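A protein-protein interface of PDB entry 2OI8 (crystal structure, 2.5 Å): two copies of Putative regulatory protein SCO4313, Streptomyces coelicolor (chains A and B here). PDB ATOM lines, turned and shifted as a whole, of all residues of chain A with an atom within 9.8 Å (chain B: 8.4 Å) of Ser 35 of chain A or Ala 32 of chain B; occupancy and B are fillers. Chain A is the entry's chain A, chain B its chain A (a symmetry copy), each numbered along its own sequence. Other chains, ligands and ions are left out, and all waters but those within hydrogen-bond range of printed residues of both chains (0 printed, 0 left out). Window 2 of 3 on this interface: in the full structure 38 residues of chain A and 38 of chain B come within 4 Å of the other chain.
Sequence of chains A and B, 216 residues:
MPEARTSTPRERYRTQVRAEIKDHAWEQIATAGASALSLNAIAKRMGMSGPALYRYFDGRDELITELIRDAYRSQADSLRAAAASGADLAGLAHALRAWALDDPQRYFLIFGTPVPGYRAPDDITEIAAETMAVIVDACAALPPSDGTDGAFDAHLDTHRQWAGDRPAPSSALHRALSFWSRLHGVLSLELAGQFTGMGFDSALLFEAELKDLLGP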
ATOM      1  N   ALA A  25      -9.517 -19.414  -8.357  1.00  0.00           N
ATOM      2  CA  ALA A  25      -8.164 -19.164  -7.860  1.00  0.00           C
ATOM      3  C   ALA A  25      -7.804 -20.155  -6.747  1.00  0.00           C
ATOM      4  O   ALA A  25      -6.696 -20.670  -6.719  1.00  0.00           O
ATOM      5  CB  ALA A  25      -8.015 -17.727  -7.385  1.00  0.00           C
ATOM      6  N   GLN A  28      -6.905 -23.567  -8.506  1.00  0.00           N
ATOM      7  CA  GLN A  28      -5.518 -23.494  -8.994  1.00  0.00           C
ATOM      8  C   GLN A  28      -4.495 -23.536  -7.871  1.00  0.00           C
ATOM      9  O   GLN A  28      -3.422 -24.113  -8.039  1.00  0.00           O
ATOM     10  CB  GLN A  28      -5.275 -22.236  -9.827  1.00  0.00           C
ATOM     11  CG  GLN A  28      -5.837 -22.266 -11.228  1.00  0.00           C
ATOM     12  CD  GLN A  28      -5.282 -21.148 -12.086  1.00  0.00           C
ATOM     13  OE1 GLN A  28      -6.003 -20.529 -12.871  1.00  0.00           O
ATOM     14  NE2 GLN A  28      -3.991 -20.879 -11.932  1.00  0.00           N
ATOM     15  N   ILE A  29      -4.807 -22.892  -6.748  1.00  0.00           N
ATOM     16  CA  ILE A  29      -3.918 -22.928  -5.581  1.00  0.00           C
ATOM     17  C   ILE A  29      -3.896 -24.367  -5.076  1.00  0.00           C
ATOM     18  O   ILE A  29      -2.832 -24.979  -4.971  1.00  0.00           O
ATOM     19  CB  ILE A  29      -4.368 -21.956  -4.450  1.00  0.00           C
ATOM     20  CG1 ILE A  29      -4.239 -20.512  -4.932  1.00  0.00           C
ATOM     21  CG2 ILE A  29      -3.557 -22.186  -3.150  1.00  0.00           C
ATOM     22  CD1 ILE A  29      -4.438 -19.511  -3.794  1.00  0.00           C
ATOM     23  N   ALA A  30      -5.089 -24.904  -4.807  1.00  0.00           N
ATOM     24  CA  ALA A  30      -5.240 -26.279  -4.348  1.00  0.00           C
ATOM     25  C   ALA A  30      -4.419 -27.232  -5.206  1.00  0.00           C
ATOM     26  O   ALA A  30      -3.531 -27.919  -4.696  1.00  0.00           O
ATOM     27  CB  ALA A  30      -6.709 -26.686  -4.331  1.00  0.00           C
ATOM     28  N   ALA A  32      -2.314 -26.631  -8.063  1.00  0.00           N
ATOM     29  CA  ALA A  32      -0.978 -26.286  -8.592  1.00  0.00           C
ATOM     30  C   ALA A  32      -0.124 -25.349  -7.730  1.00  0.00           C
ATOM     31  O   ALA A  32       1.031 -25.062  -8.074  1.00  0.00           O
ATOM     32  CB  ALA A  32      -1.096 -25.737 -10.014  1.00  0.00           C
ATOM     33  N   GLY A  33      -0.689 -24.878  -6.620  1.00  0.00           N
ATOM     34  CA  GLY A  33       0.036 -24.034  -5.676  1.00  0.00           C
ATOM     35  C   GLY A  33       0.033 -22.569  -6.055  1.00  0.00           C
ATOM     36  O   GLY A  33       0.136 -22.210  -7.233  1.00  0.00           O
ATOM     37  N   ALA A  34      -0.089 -21.714  -5.047  1.00  0.00           N
ATOM     38  CA  ALA A  34       0.052 -20.278  -5.254  1.00  0.00           C
ATOM     39  C   ALA A  34       1.326 -20.054  -6.063  1.00  0.00           C
ATOM     40  O   ALA A  34       2.209 -20.920  -6.074  1.00  0.00           O
ATOM     41  CB  ALA A  34       0.131 -19.567  -3.917  1.00  0.00           C
ATOM     42  N   SER A  35       1.434 -18.923  -6.760  1.00  0.00           N
ATOM     43  CA  SER A  35       2.672 -18.611  -7.537  1.00  0.00           C
ATOM     44  C   SER A  35       2.613 -19.216  -8.936  1.00  0.00           C
ATOM     45  O   SER A  35       2.843 -18.515  -9.925  1.00  0.00           O
ATOM     46  CB  SER A  35       3.954 -19.060  -6.807  1.00  0.00           C
ATOM     47  OG  SER A  35       5.128 -18.507  -7.387  1.00  0.00           O
ATOM     48  N   ALA A  36       2.298 -20.512  -9.010  1.00  0.00           N
ATOM     49  CA  ALA A  36       1.871 -21.123 -10.265  1.00  0.00           C
ATOM     50  C   ALA A  36       0.514 -20.553 -10.643  1.00  0.00           C
ATOM     51  O   ALA A  36       0.059 -20.716 -11.774  1.00  0.00           O
ATOM     52  CB  ALA A  36       1.796 -22.633 -10.131  1.00  0.00           C
ATOM     53  N   LEU A  37      -0.126 -19.881  -9.690  1.00  0.00           N
ATOM     54  CA  LEU A  37      -1.453 -19.281  -9.890  1.00  0.00           C
ATOM     55  C   LEU A  37      -1.467 -18.195 -10.976  1.00  0.00           C
ATOM     56  O   LEU A  37      -0.709 -17.234 -10.902  1.00  0.00           O
ATOM     57  CB  LEU A  37      -1.940 -18.717  -8.553  1.00  0.00           C
ATOM     58  CG  LEU A  37      -3.111 -17.740  -8.478  1.00  0.00           C
ATOM     59  CD1 LEU A  37      -4.410 -18.349  -9.026  1.00  0.00           C
ATOM     60  CD2 LEU A  37      -3.278 -17.306  -7.040  1.00  0.00           C
ATOM     61  N   SER A  38      -2.339 -18.335 -11.972  1.00  0.00           N
ATOM     62  CA  SER A  38      -2.320 -17.432 -13.132  1.00  0.00           C
ATOM     63  C   SER A  38      -3.687 -16.977 -13.656  1.00  0.00           C
ATOM     64  O   SER A  38      -4.544 -17.794 -13.980  1.00  0.00           O
ATOM     65  CB  SER A  38      -1.530 -18.067 -14.280  1.00  0.00           C
ATOM     66  OG  SER A  38      -2.306 -19.040 -14.955  1.00  0.00           O
ATOM     67  N   LEU A  39      -3.852 -15.665 -13.778  1.00  0.00           N
ATOM     68  CA  LEU A  39      -5.064 -15.062 -14.314  1.00  0.00           C
ATOM     69  C   LEU A  39      -5.436 -15.556 -15.708  1.00  0.00           C
ATOM     70  O   LEU A  39      -6.612 -15.543 -16.080  1.00  0.00           O
ATOM     71  CB  LEU A  39      -4.954 -13.545 -14.319  1.00  0.00           C
ATOM     72  CG  LEU A  39      -5.045 -12.869 -12.955  1.00  0.00           C
ATOM     73  CD1 LEU A  39      -4.725 -11.401 -13.086  1.00  0.00           C
ATOM     74  CD2 LEU A  39      -6.433 -13.031 -12.394  1.00  0.00           C
ATOM     75  N   ARG A  60      -1.672 -10.688 -10.858  1.00  0.00           N
ATOM     76  CA  ARG A  60      -1.682 -11.767  -9.900  1.00  0.00           C
ATOM     77  C   ARG A  60      -1.558 -11.319  -8.438  1.00  0.00           C
ATOM     78  O   ARG A  60      -2.119 -11.955  -7.540  1.00  0.00           O
ATOM     79  CB  ARG A  60      -0.582 -12.787 -10.252  1.00  0.00           C
ATOM     80  CG  ARG A  60      -0.326 -13.905  -9.186  1.00  0.00           C
ATOM     81  CD  ARG A  60       0.866 -14.776  -9.591  1.00  0.00           C
ATOM     82  NE  ARG A  60       1.861 -14.988  -8.523  1.00  0.00           N
ATOM     83  CZ  ARG A  60       2.798 -14.097  -8.199  1.00  0.00           C
ATOM     84  NH1 ARG A  60       2.845 -12.930  -8.819  1.00  0.00           N
ATOM     85  NH2 ARG A  60       3.681 -14.347  -7.254  1.00  0.00           N
ATOM     86  N   ASP A  61      -0.814 -10.247  -8.183  1.00  0.00           N
ATOM     87  CA  ASP A  61      -0.586  -9.844  -6.788  1.00  0.00           C
ATOM     88  C   ASP A  61      -1.832  -9.226  -6.198  1.00  0.00           C
ATOM     89  O   ASP A  61      -2.143  -9.469  -5.040  1.00  0.00           O
ATOM     90  CB  ASP A  61       0.603  -8.890  -6.647  1.00  0.00           C
ATOM     91  CG  ASP A  61       1.955  -9.588  -6.843  1.00  0.00           C
ATOM     92  OD1 ASP A  61       2.032 -10.836  -6.725  1.00  0.00           O
ATOM     93  OD2 ASP A  61       2.939  -8.867  -7.132  1.00  0.00           O
ATOM     94  N   LEU A  63      -4.814 -10.130  -7.030  1.00  0.00           N
ATOM     95  CA  LEU A  63      -5.655 -11.253  -6.743  1.00  0.00           C
ATOM     96  C   LEU A  63      -5.187 -11.919  -5.464  1.00  0.00           C
ATOM     97  O   LEU A  63      -6.005 -12.200  -4.595  1.00  0.00           O
ATOM     98  CB  LEU A  63      -5.654 -12.247  -7.894  1.00  0.00           C
ATOM     99  CG  LEU A  63      -6.460 -13.523  -7.614  1.00  0.00           C
ATOM    100  CD1 LEU A  63      -7.953 -13.264  -7.277  1.00  0.00           C
ATOM    101  CD2 LEU A  63      -6.340 -14.459  -8.798  1.00  0.00           C
ATOM    102  N   ILE A  64      -3.877 -12.157  -5.337  1.00  0.00           N
ATOM    103  CA  ILE A  64      -3.346 -12.800  -4.141  1.00  0.00           C
ATOM    104  C   ILE A  64      -3.757 -11.957  -2.943  1.00  0.00           C
ATOM    105  O   ILE A  64      -4.355 -12.476  -1.974  1.00  0.00           O
ATOM    106  CB  ILE A  64      -1.797 -12.900  -4.148  1.00  0.00           C
ATOM    107  CG1 ILE A  64      -1.253 -13.824  -5.257  1.00  0.00           C
ATOM    108  CG2 ILE A  64      -1.274 -13.276  -2.748  1.00  0.00           C
ATOM    109  CD1 ILE A  64      -1.626 -15.246  -5.106  1.00  0.00           C
ATOM    110  N   LEU A  67      -7.254 -12.519  -1.832  1.00  0.00           N
ATOM    111  CA  LEU A  67      -7.384 -13.829  -1.207  1.00  0.00           C
ATOM    112  C   LEU A  67      -6.812 -13.782   0.222  1.00  0.00           C
ATOM    113  O   LEU A  67      -7.456 -14.242   1.158  1.00  0.00           O
ATOM    114  CB  LEU A  67      -6.701 -14.909  -2.051  1.00  0.00           C
ATOM    115  CG  LEU A  67      -7.210 -15.166  -3.480  1.00  0.00           C
ATOM    116  CD1 LEU A  67      -6.342 -16.236  -4.102  1.00  0.00           C
ATOM    117  CD2 LEU A  67      -8.696 -15.572  -3.548  1.00  0.00           C
ATOM    118  N   LEU A 109      -2.275 -20.228   3.150  1.00  0.00           N
ATOM    119  CA  LEU A 109      -2.046 -19.002   2.412  1.00  0.00           C
ATOM    120  C   LEU A 109      -1.573 -17.894   3.400  1.00  0.00           C
ATOM    121  O   LEU A 109      -0.720 -17.078   3.069  1.00  0.00           O
ATOM    122  CB  LEU A 109      -3.316 -18.630   1.632  1.00  0.00           C
ATOM    123  CG  LEU A 109      -3.222 -17.461   0.636  1.00  0.00           C
ATOM    124  CD1 LEU A 109      -2.466 -17.795  -0.678  1.00  0.00           C
ATOM    125  CD2 LEU A 109      -4.602 -16.916   0.342  1.00  0.00           C
ATOM    126  N   THR A 113       3.828 -21.529   3.556  1.00  0.00           N
ATOM    127  CA  THR A 113       4.919 -21.105   2.723  1.00  0.00           C
ATOM    128  C   THR A 113       4.577 -19.807   1.993  1.00  0.00           C
ATOM    129  O   THR A 113       3.595 -19.747   1.263  1.00  0.00           O
ATOM    130  CB  THR A 113       5.248 -22.230   1.738  1.00  0.00           C
ATOM    131  OG1 THR A 113       5.384 -23.453   2.481  1.00  0.00           O
ATOM    132  CG2 THR A 113       6.535 -21.920   0.933  1.00  0.00           C
ATOM    133  N   PRO A 114       5.408 -18.768   2.168  1.00  0.00           N
ATOM    134  CA  PRO A 114       5.145 -17.477   1.528  1.00  0.00           C
ATOM    135  C   PRO A 114       5.093 -17.631  -0.001  1.00  0.00           C
ATOM    136  O   PRO A 114       5.740 -18.525  -0.558  1.00  0.00           O
ATOM    137  CB  PRO A 114       6.375 -16.627   1.891  1.00  0.00           C
ATOM    138  CG  PRO A 114       7.163 -17.386   2.905  1.00  0.00           C
ATOM    139  CD  PRO A 114       6.682 -18.807   2.908  1.00  0.00           C
ATOM    140  N   VAL A 115       4.353 -16.770  -0.691  1.00  0.00           N
ATOM    141  CA  VAL A 115       4.305 -16.891  -2.139  1.00  0.00           C
ATOM    142  C   VAL A 115       5.493 -16.149  -2.735  1.00  0.00           C
ATOM    143  O   VAL A 115       5.669 -14.968  -2.477  1.00  0.00           O
ATOM    144  CB  VAL A 115       2.968 -16.414  -2.709  1.00  0.00           C
ATOM    145  CG1 VAL A 115       2.955 -16.576  -4.221  1.00  0.00           C
ATOM    146  CG2 VAL A 115       1.848 -17.188  -2.064  1.00  0.00           C
ATOM    147  N   PRO A 116       6.349 -16.869  -3.488  1.00  0.00           N
ATOM    148  CA  PRO A 116       7.585 -16.293  -4.025  1.00  0.00           C
ATOM    149  C   PRO A 116       7.275 -15.149  -4.934  1.00  0.00           C
ATOM    150  O   PRO A 116       6.380 -15.256  -5.768  1.00  0.00           O
ATOM    151  CB  PRO A 116       8.180 -17.430  -4.853  1.00  0.00           C
ATOM    152  CG  PRO A 116       7.607 -18.658  -4.267  1.00  0.00           C
ATOM    153  CD  PRO A 116       6.207 -18.289  -3.865  1.00  0.00           C
ATOM    154  N   GLY A 117       8.011 -14.059  -4.755  1.00  0.00           N
ATOM    155  CA  GLY A 117       7.860 -12.877  -5.593  1.00  0.00           C
ATOM    156  C   GLY A 117       6.812 -11.896  -5.085  1.00  0.00           C
ATOM    157  O   GLY A 117       6.889 -10.697  -5.400  1.00  0.00           O
ATOM    158  N   TYR A 118       5.847 -12.390  -4.299  1.00  0.00           N
ATOM    159  CA  TYR A 118       4.736 -11.567  -3.838  1.00  0.00           C
ATOM    160  C   TYR A 118       5.096 -10.738  -2.608  1.00  0.00           C
ATOM    161  O   TYR A 118       5.498 -11.289  -1.575  1.00  0.00           O
ATOM    162  CB  TYR A 118       3.500 -12.435  -3.531  1.00  0.00           C
ATOM    163  CG  TYR A 118       2.401 -11.681  -2.819  1.00  0.00           C
ATOM    164  CD1 TYR A 118       1.508 -10.887  -3.527  1.00  0.00           C
ATOM    165  CD2 TYR A 118       2.268 -11.744  -1.436  1.00  0.00           C
ATOM    166  CE1 TYR A 118       0.498 -10.177  -2.887  1.00  0.00           C
ATOM    167  CE2 TYR A 118       1.256 -11.046  -0.776  1.00  0.00           C
ATOM    168  CZ  TYR A 118       0.367 -10.259  -1.513  1.00  0.00           C
ATOM    169  OH  TYR A 118      -0.634  -9.547  -0.877  1.00  0.00           O
ATOM    170  N   ALA B  25      17.002 -27.597  -8.187  1.00  0.00           N
ATOM    171  CA  ALA B  25      15.642 -27.848  -7.709  1.00  0.00           C
ATOM    172  C   ALA B  25      15.267 -26.861  -6.598  1.00  0.00           C
ATOM    173  O   ALA B  25      14.159 -26.346  -6.584  1.00  0.00           O
ATOM    174  CB  ALA B  25      15.486 -29.286  -7.241  1.00  0.00           C
ATOM    175  N   TRP B  26      16.193 -26.564  -5.692  1.00  0.00           N
ATOM    176  CA  TRP B  26      15.924 -25.534  -4.707  1.00  0.00           C
ATOM    177  C   TRP B  26      15.649 -24.186  -5.387  1.00  0.00           C
ATOM    178  O   TRP B  26      14.673 -23.519  -5.027  1.00  0.00           O
ATOM    179  CB  TRP B  26      17.029 -25.450  -3.649  1.00  0.00           C
ATOM    180  CG  TRP B  26      17.053 -26.676  -2.764  1.00  0.00           C
ATOM    181  CD1 TRP B  26      17.949 -27.724  -2.814  1.00  0.00           C
ATOM    182  CD2 TRP B  26      16.120 -27.003  -1.711  1.00  0.00           C
ATOM    183  NE1 TRP B  26      17.633 -28.669  -1.849  1.00  0.00           N
ATOM    184  CE2 TRP B  26      16.522 -28.252  -1.164  1.00  0.00           C
ATOM    185  CE3 TRP B  26      14.995 -26.355  -1.170  1.00  0.00           C
ATOM    186  CZ2 TRP B  26      15.836 -28.862  -0.119  1.00  0.00           C
ATOM    187  CZ3 TRP B  26      14.317 -26.968  -0.135  1.00  0.00           C
ATOM    188  CH2 TRP B  26      14.742 -28.203   0.382  1.00  0.00           C
ATOM    189  N   GLU B  27      16.464 -23.810  -6.384  1.00  0.00           N
ATOM    190  CA  GLU B  27      16.278 -22.536  -7.114  1.00  0.00           C
ATOM    191  C   GLU B  27      14.839 -22.419  -7.618  1.00  0.00           C
ATOM    192  O   GLU B  27      14.146 -21.430  -7.318  1.00  0.00           O
ATOM    193  CB  GLU B  27      17.258 -22.380  -8.292  1.00  0.00           C
ATOM    194  CG  GLU B  27      18.674 -21.982  -7.912  1.00  0.00           C
ATOM    195  CD  GLU B  27      19.685 -22.058  -9.097  1.00  0.00           C
ATOM    196  OE1 GLU B  27      19.553 -22.905 -10.031  1.00  0.00           O
ATOM    197  OE2 GLU B  27      20.636 -21.256  -9.076  1.00  0.00           O
ATOM    198  N   GLN B  28      14.392 -23.443  -8.360  1.00  0.00           N
ATOM    199  CA  GLN B  28      13.011 -23.515  -8.866  1.00  0.00           C
ATOM    200  C   GLN B  28      11.974 -23.476  -7.758  1.00  0.00           C
ATOM    201  O   GLN B  28      10.903 -22.898  -7.939  1.00  0.00           O
ATOM    202  CB  GLN B  28      12.781 -24.770  -9.706  1.00  0.00           C
ATOM    203  CG  GLN B  28      13.361 -24.736 -11.100  1.00  0.00           C
ATOM    204  CD  GLN B  28      12.819 -25.852 -11.969  1.00  0.00           C
ATOM    205  OE1 GLN B  28      13.550 -26.468 -12.746  1.00  0.00           O
ATOM    206  NE2 GLN B  28      11.526 -26.121 -11.833  1.00  0.00           N
ATOM    207  N   ILE B  29      12.270 -24.124  -6.633  1.00  0.00           N
ATOM    208  CA  ILE B  29      11.365 -24.090  -5.477  1.00  0.00           C
ATOM    209  C   ILE B  29      11.336 -22.654  -4.968  1.00  0.00           C
ATOM    210  O   ILE B  29      10.271 -22.041  -4.877  1.00  0.00           O
ATOM    211  CB  ILE B  29      11.799 -25.066  -4.344  1.00  0.00           C
ATOM    212  CG1 ILE B  29      11.677 -26.509  -4.832  1.00  0.00           C
ATOM    213  CG2 ILE B  29      10.970 -24.839  -3.054  1.00  0.00           C
ATOM    214  CD1 ILE B  29      11.861 -27.513  -3.695  1.00  0.00           C
ATOM    215  N   ALA B  30      12.525 -22.117  -4.682  1.00  0.00           N
ATOM    216  CA  ALA B  30      12.670 -20.744  -4.217  1.00  0.00           C
ATOM    217  C   ALA B  30      11.861 -19.787  -5.083  1.00  0.00           C
ATOM    218  O   ALA B  30      10.965 -19.103  -4.583  1.00  0.00           O
ATOM    219  CB  ALA B  30      14.139 -20.336  -4.178  1.00  0.00           C
ATOM    220  N   THR B  31      12.139 -19.779  -6.381  1.00  0.00           N
ATOM    221  CA  THR B  31      11.533 -18.797  -7.270  1.00  0.00           C
ATOM    222  C   THR B  31      10.095 -19.122  -7.670  1.00  0.00           C
ATOM    223  O   THR B  31       9.254 -18.246  -7.660  1.00  0.00           O
ATOM    224  CB  THR B  31      12.434 -18.457  -8.514  1.00  0.00           C
ATOM    225  OG1 THR B  31      13.201 -19.602  -8.904  1.00  0.00           O
ATOM    226  CG2 THR B  31      13.402 -17.308  -8.191  1.00  0.00           C
ATOM    227  N   ALA B  32       9.795 -20.380  -7.970  1.00  0.00           N
ATOM    228  CA  ALA B  32       8.467 -20.723  -8.519  1.00  0.00           C
ATOM    229  C   ALA B  32       7.601 -21.663  -7.672  1.00  0.00           C
ATOM    230  O   ALA B  32       6.451 -21.950  -8.032  1.00  0.00           O
ATOM    231  CB  ALA B  32       8.605 -21.269  -9.941  1.00  0.00           C
ATOM    232  N   GLY B  33       8.150 -22.138  -6.555  1.00  0.00           N
ATOM    233  CA  GLY B  33       7.412 -22.984  -5.624  1.00  0.00           C
ATOM    234  C   GLY B  33       7.421 -24.448  -6.007  1.00  0.00           C
ATOM    235  O   GLY B  33       7.334 -24.804  -7.188  1.00  0.00           O
ATOM    236  N   ALA B  34       7.529 -25.306  -5.000  1.00  0.00           N
ATOM    237  CA  ALA B  34       7.391 -26.741  -5.213  1.00  0.00           C
ATOM    238  C   ALA B  34       6.129 -26.963  -6.040  1.00  0.00           C
ATOM    239  O   ALA B  34       5.245 -26.098  -6.060  1.00  0.00           O
ATOM    240  CB  ALA B  34       7.294 -27.457  -3.879  1.00  0.00           C
ATOM    241  N   SER B  35       6.030 -28.092  -6.743  1.00  0.00           N
ATOM    242  CA  SER B  35       4.802 -28.402  -7.537  1.00  0.00           C
ATOM    243  C   SER B  35       4.880 -27.792  -8.933  1.00  0.00           C
ATOM    244  O   SER B  35       4.664 -28.490  -9.927  1.00  0.00           O
ATOM    245  CB  SER B  35       3.511 -27.956  -6.823  1.00  0.00           C
ATOM    246  OG  SER B  35       2.344 -28.506  -7.420  1.00  0.00           O
ATOM    247  N   ALA B  36       5.196 -26.496  -8.999  1.00  0.00           N
ATOM    248  CA  ALA B  36       5.641 -25.882 -10.246  1.00  0.00           C
ATOM    249  C   ALA B  36       7.003 -26.450 -10.607  1.00  0.00           C
ATOM    250  O   ALA B  36       7.474 -26.284 -11.731  1.00  0.00           O
ATOM    251  CB  ALA B  36       5.714 -24.372 -10.107  1.00  0.00           C
ATOM    252  N   LEU B  37       7.630 -27.125  -9.647  1.00  0.00           N
ATOM    253  CA  LEU B  37       8.959 -27.724  -9.831  1.00  0.00           C
ATOM    254  C   LEU B  37       8.988 -28.808 -10.921  1.00  0.00           C
ATOM    255  O   LEU B  37       8.230 -29.769 -10.859  1.00  0.00           O
ATOM    256  CB  LEU B  37       9.429 -28.293  -8.489  1.00  0.00           C
ATOM    257  CG  LEU B  37      10.598 -29.270  -8.401  1.00  0.00           C
ATOM    258  CD1 LEU B  37      11.905 -28.659  -8.929  1.00  0.00           C
ATOM    259  CD2 LEU B  37      10.745 -29.708  -6.963  1.00  0.00           C
ATOM    260  N   SER B  38       9.875 -28.664 -11.904  1.00  0.00           N
ATOM    261  CA  SER B  38       9.871 -29.564 -13.066  1.00  0.00           C
ATOM    262  C   SER B  38      11.245 -30.017 -13.573  1.00  0.00           C
ATOM    263  O   SER B  38      12.107 -29.199 -13.883  1.00  0.00           O
ATOM    264  CB  SER B  38       9.097 -28.926 -14.224  1.00  0.00           C
ATOM    265  OG  SER B  38       9.882 -27.951 -14.884  1.00  0.00           O
ATOM    266  N   GLN B 105      13.450 -22.000   3.175  1.00  0.00           N
ATOM    267  CA  GLN B 105      12.859 -22.799   2.112  1.00  0.00           C
ATOM    268  C   GLN B 105      12.909 -24.253   2.496  1.00  0.00           C
ATOM    269  O   GLN B 105      11.937 -24.987   2.284  1.00  0.00           O
ATOM    270  CB  GLN B 105      13.558 -22.588   0.769  1.00  0.00           C
ATOM    271  CG  GLN B 105      13.326 -21.241   0.166  1.00  0.00           C
ATOM    272  CD  GLN B 105      11.850 -20.889   0.080  1.00  0.00           C
ATOM    273  OE1 GLN B 105      11.022 -21.643  -0.474  1.00  0.00           O
ATOM    274  NE2 GLN B 105      11.505 -19.735   0.633  1.00  0.00           N
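The guanidinium group (NH2) of Arg 60 of chain A sits at hydrogen-bond distance from the backbone carbonyl oxygen (O) of Pro 116 of chain A, 3.2 Å away.
O of Glu 27 of chain B lies within hydrogen-bond range of OG1 of Thr 31 of chain B (2.6 Å).
Ser 35 of chain B touches Ala 32 of chain A (OG to O, 3.7 Å).
O of Ala 32 of chain B touches OG of Ser 35 of chain A (3.7 Å).
Pro 116 of chain A touches Ala 30 of chain B (CB to O, 3.3 Å).
Pro 116 of chain A touches Thr 31 of chain B (CB to O, 3.1 Å).
Ile 29 of chain A touches none of the printed residues of chain B.
Of the printed residues of chain B, Ala 32 of chain A touches Ser 35.
Ala 34 of chain A touches none of the printed residues of chain B.
Printed residues of chain B within 4 Å of Ser 35 of chain A: Ala 32.
Ala 36 of chain A touches none of the printed residues of chain B.
Leu 39 of chain A touches none of the printed residues of chain B.
Of the printed residues of chain B, Pro 116 of chain A touches Ala 30 and Thr 31.
Printed residues of chain A within 4 Å of Ala 30 of chain B: Pro 116.
Ala 32 of chain B touches just one residue of chain A: Ser 35 (3.7 Å).
Printed residues of chain A within 4 Å of Ser 35 of chain B: Ala 32.
No residue of chain A comes within 4 Å of Ala 36 of chain B.
The nearest residue of chain B that does not touch Ser 35 of chain A is Thr 31 of chain B (4.1 Å).
Of the 15 printed residues of chain B, 4 touch a printed residue of chain A.
Printed residues of chain B that touch a printed residue of chain A: Ala 30, Thr 31, Ala 32 and Ser 35.
Among the printed residues, no Asp or Glu carboxylate lies within 4 Å of a Lys or Arg side-chain nitrogen of the other chain.
Ala 32 of chain A touches Ser 35 of chain B, and with the chains exchanged Ser 35 of chain A touches Ala 32 of chain B.
Positions printed for both chains: 25, 28, 29, 30, 32, 33, 34, 35, 36, 37 and 38.
Of the 4 pairs that touch across the chains among the printed residues, 2 have their exchanged pair printed and touching as well.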
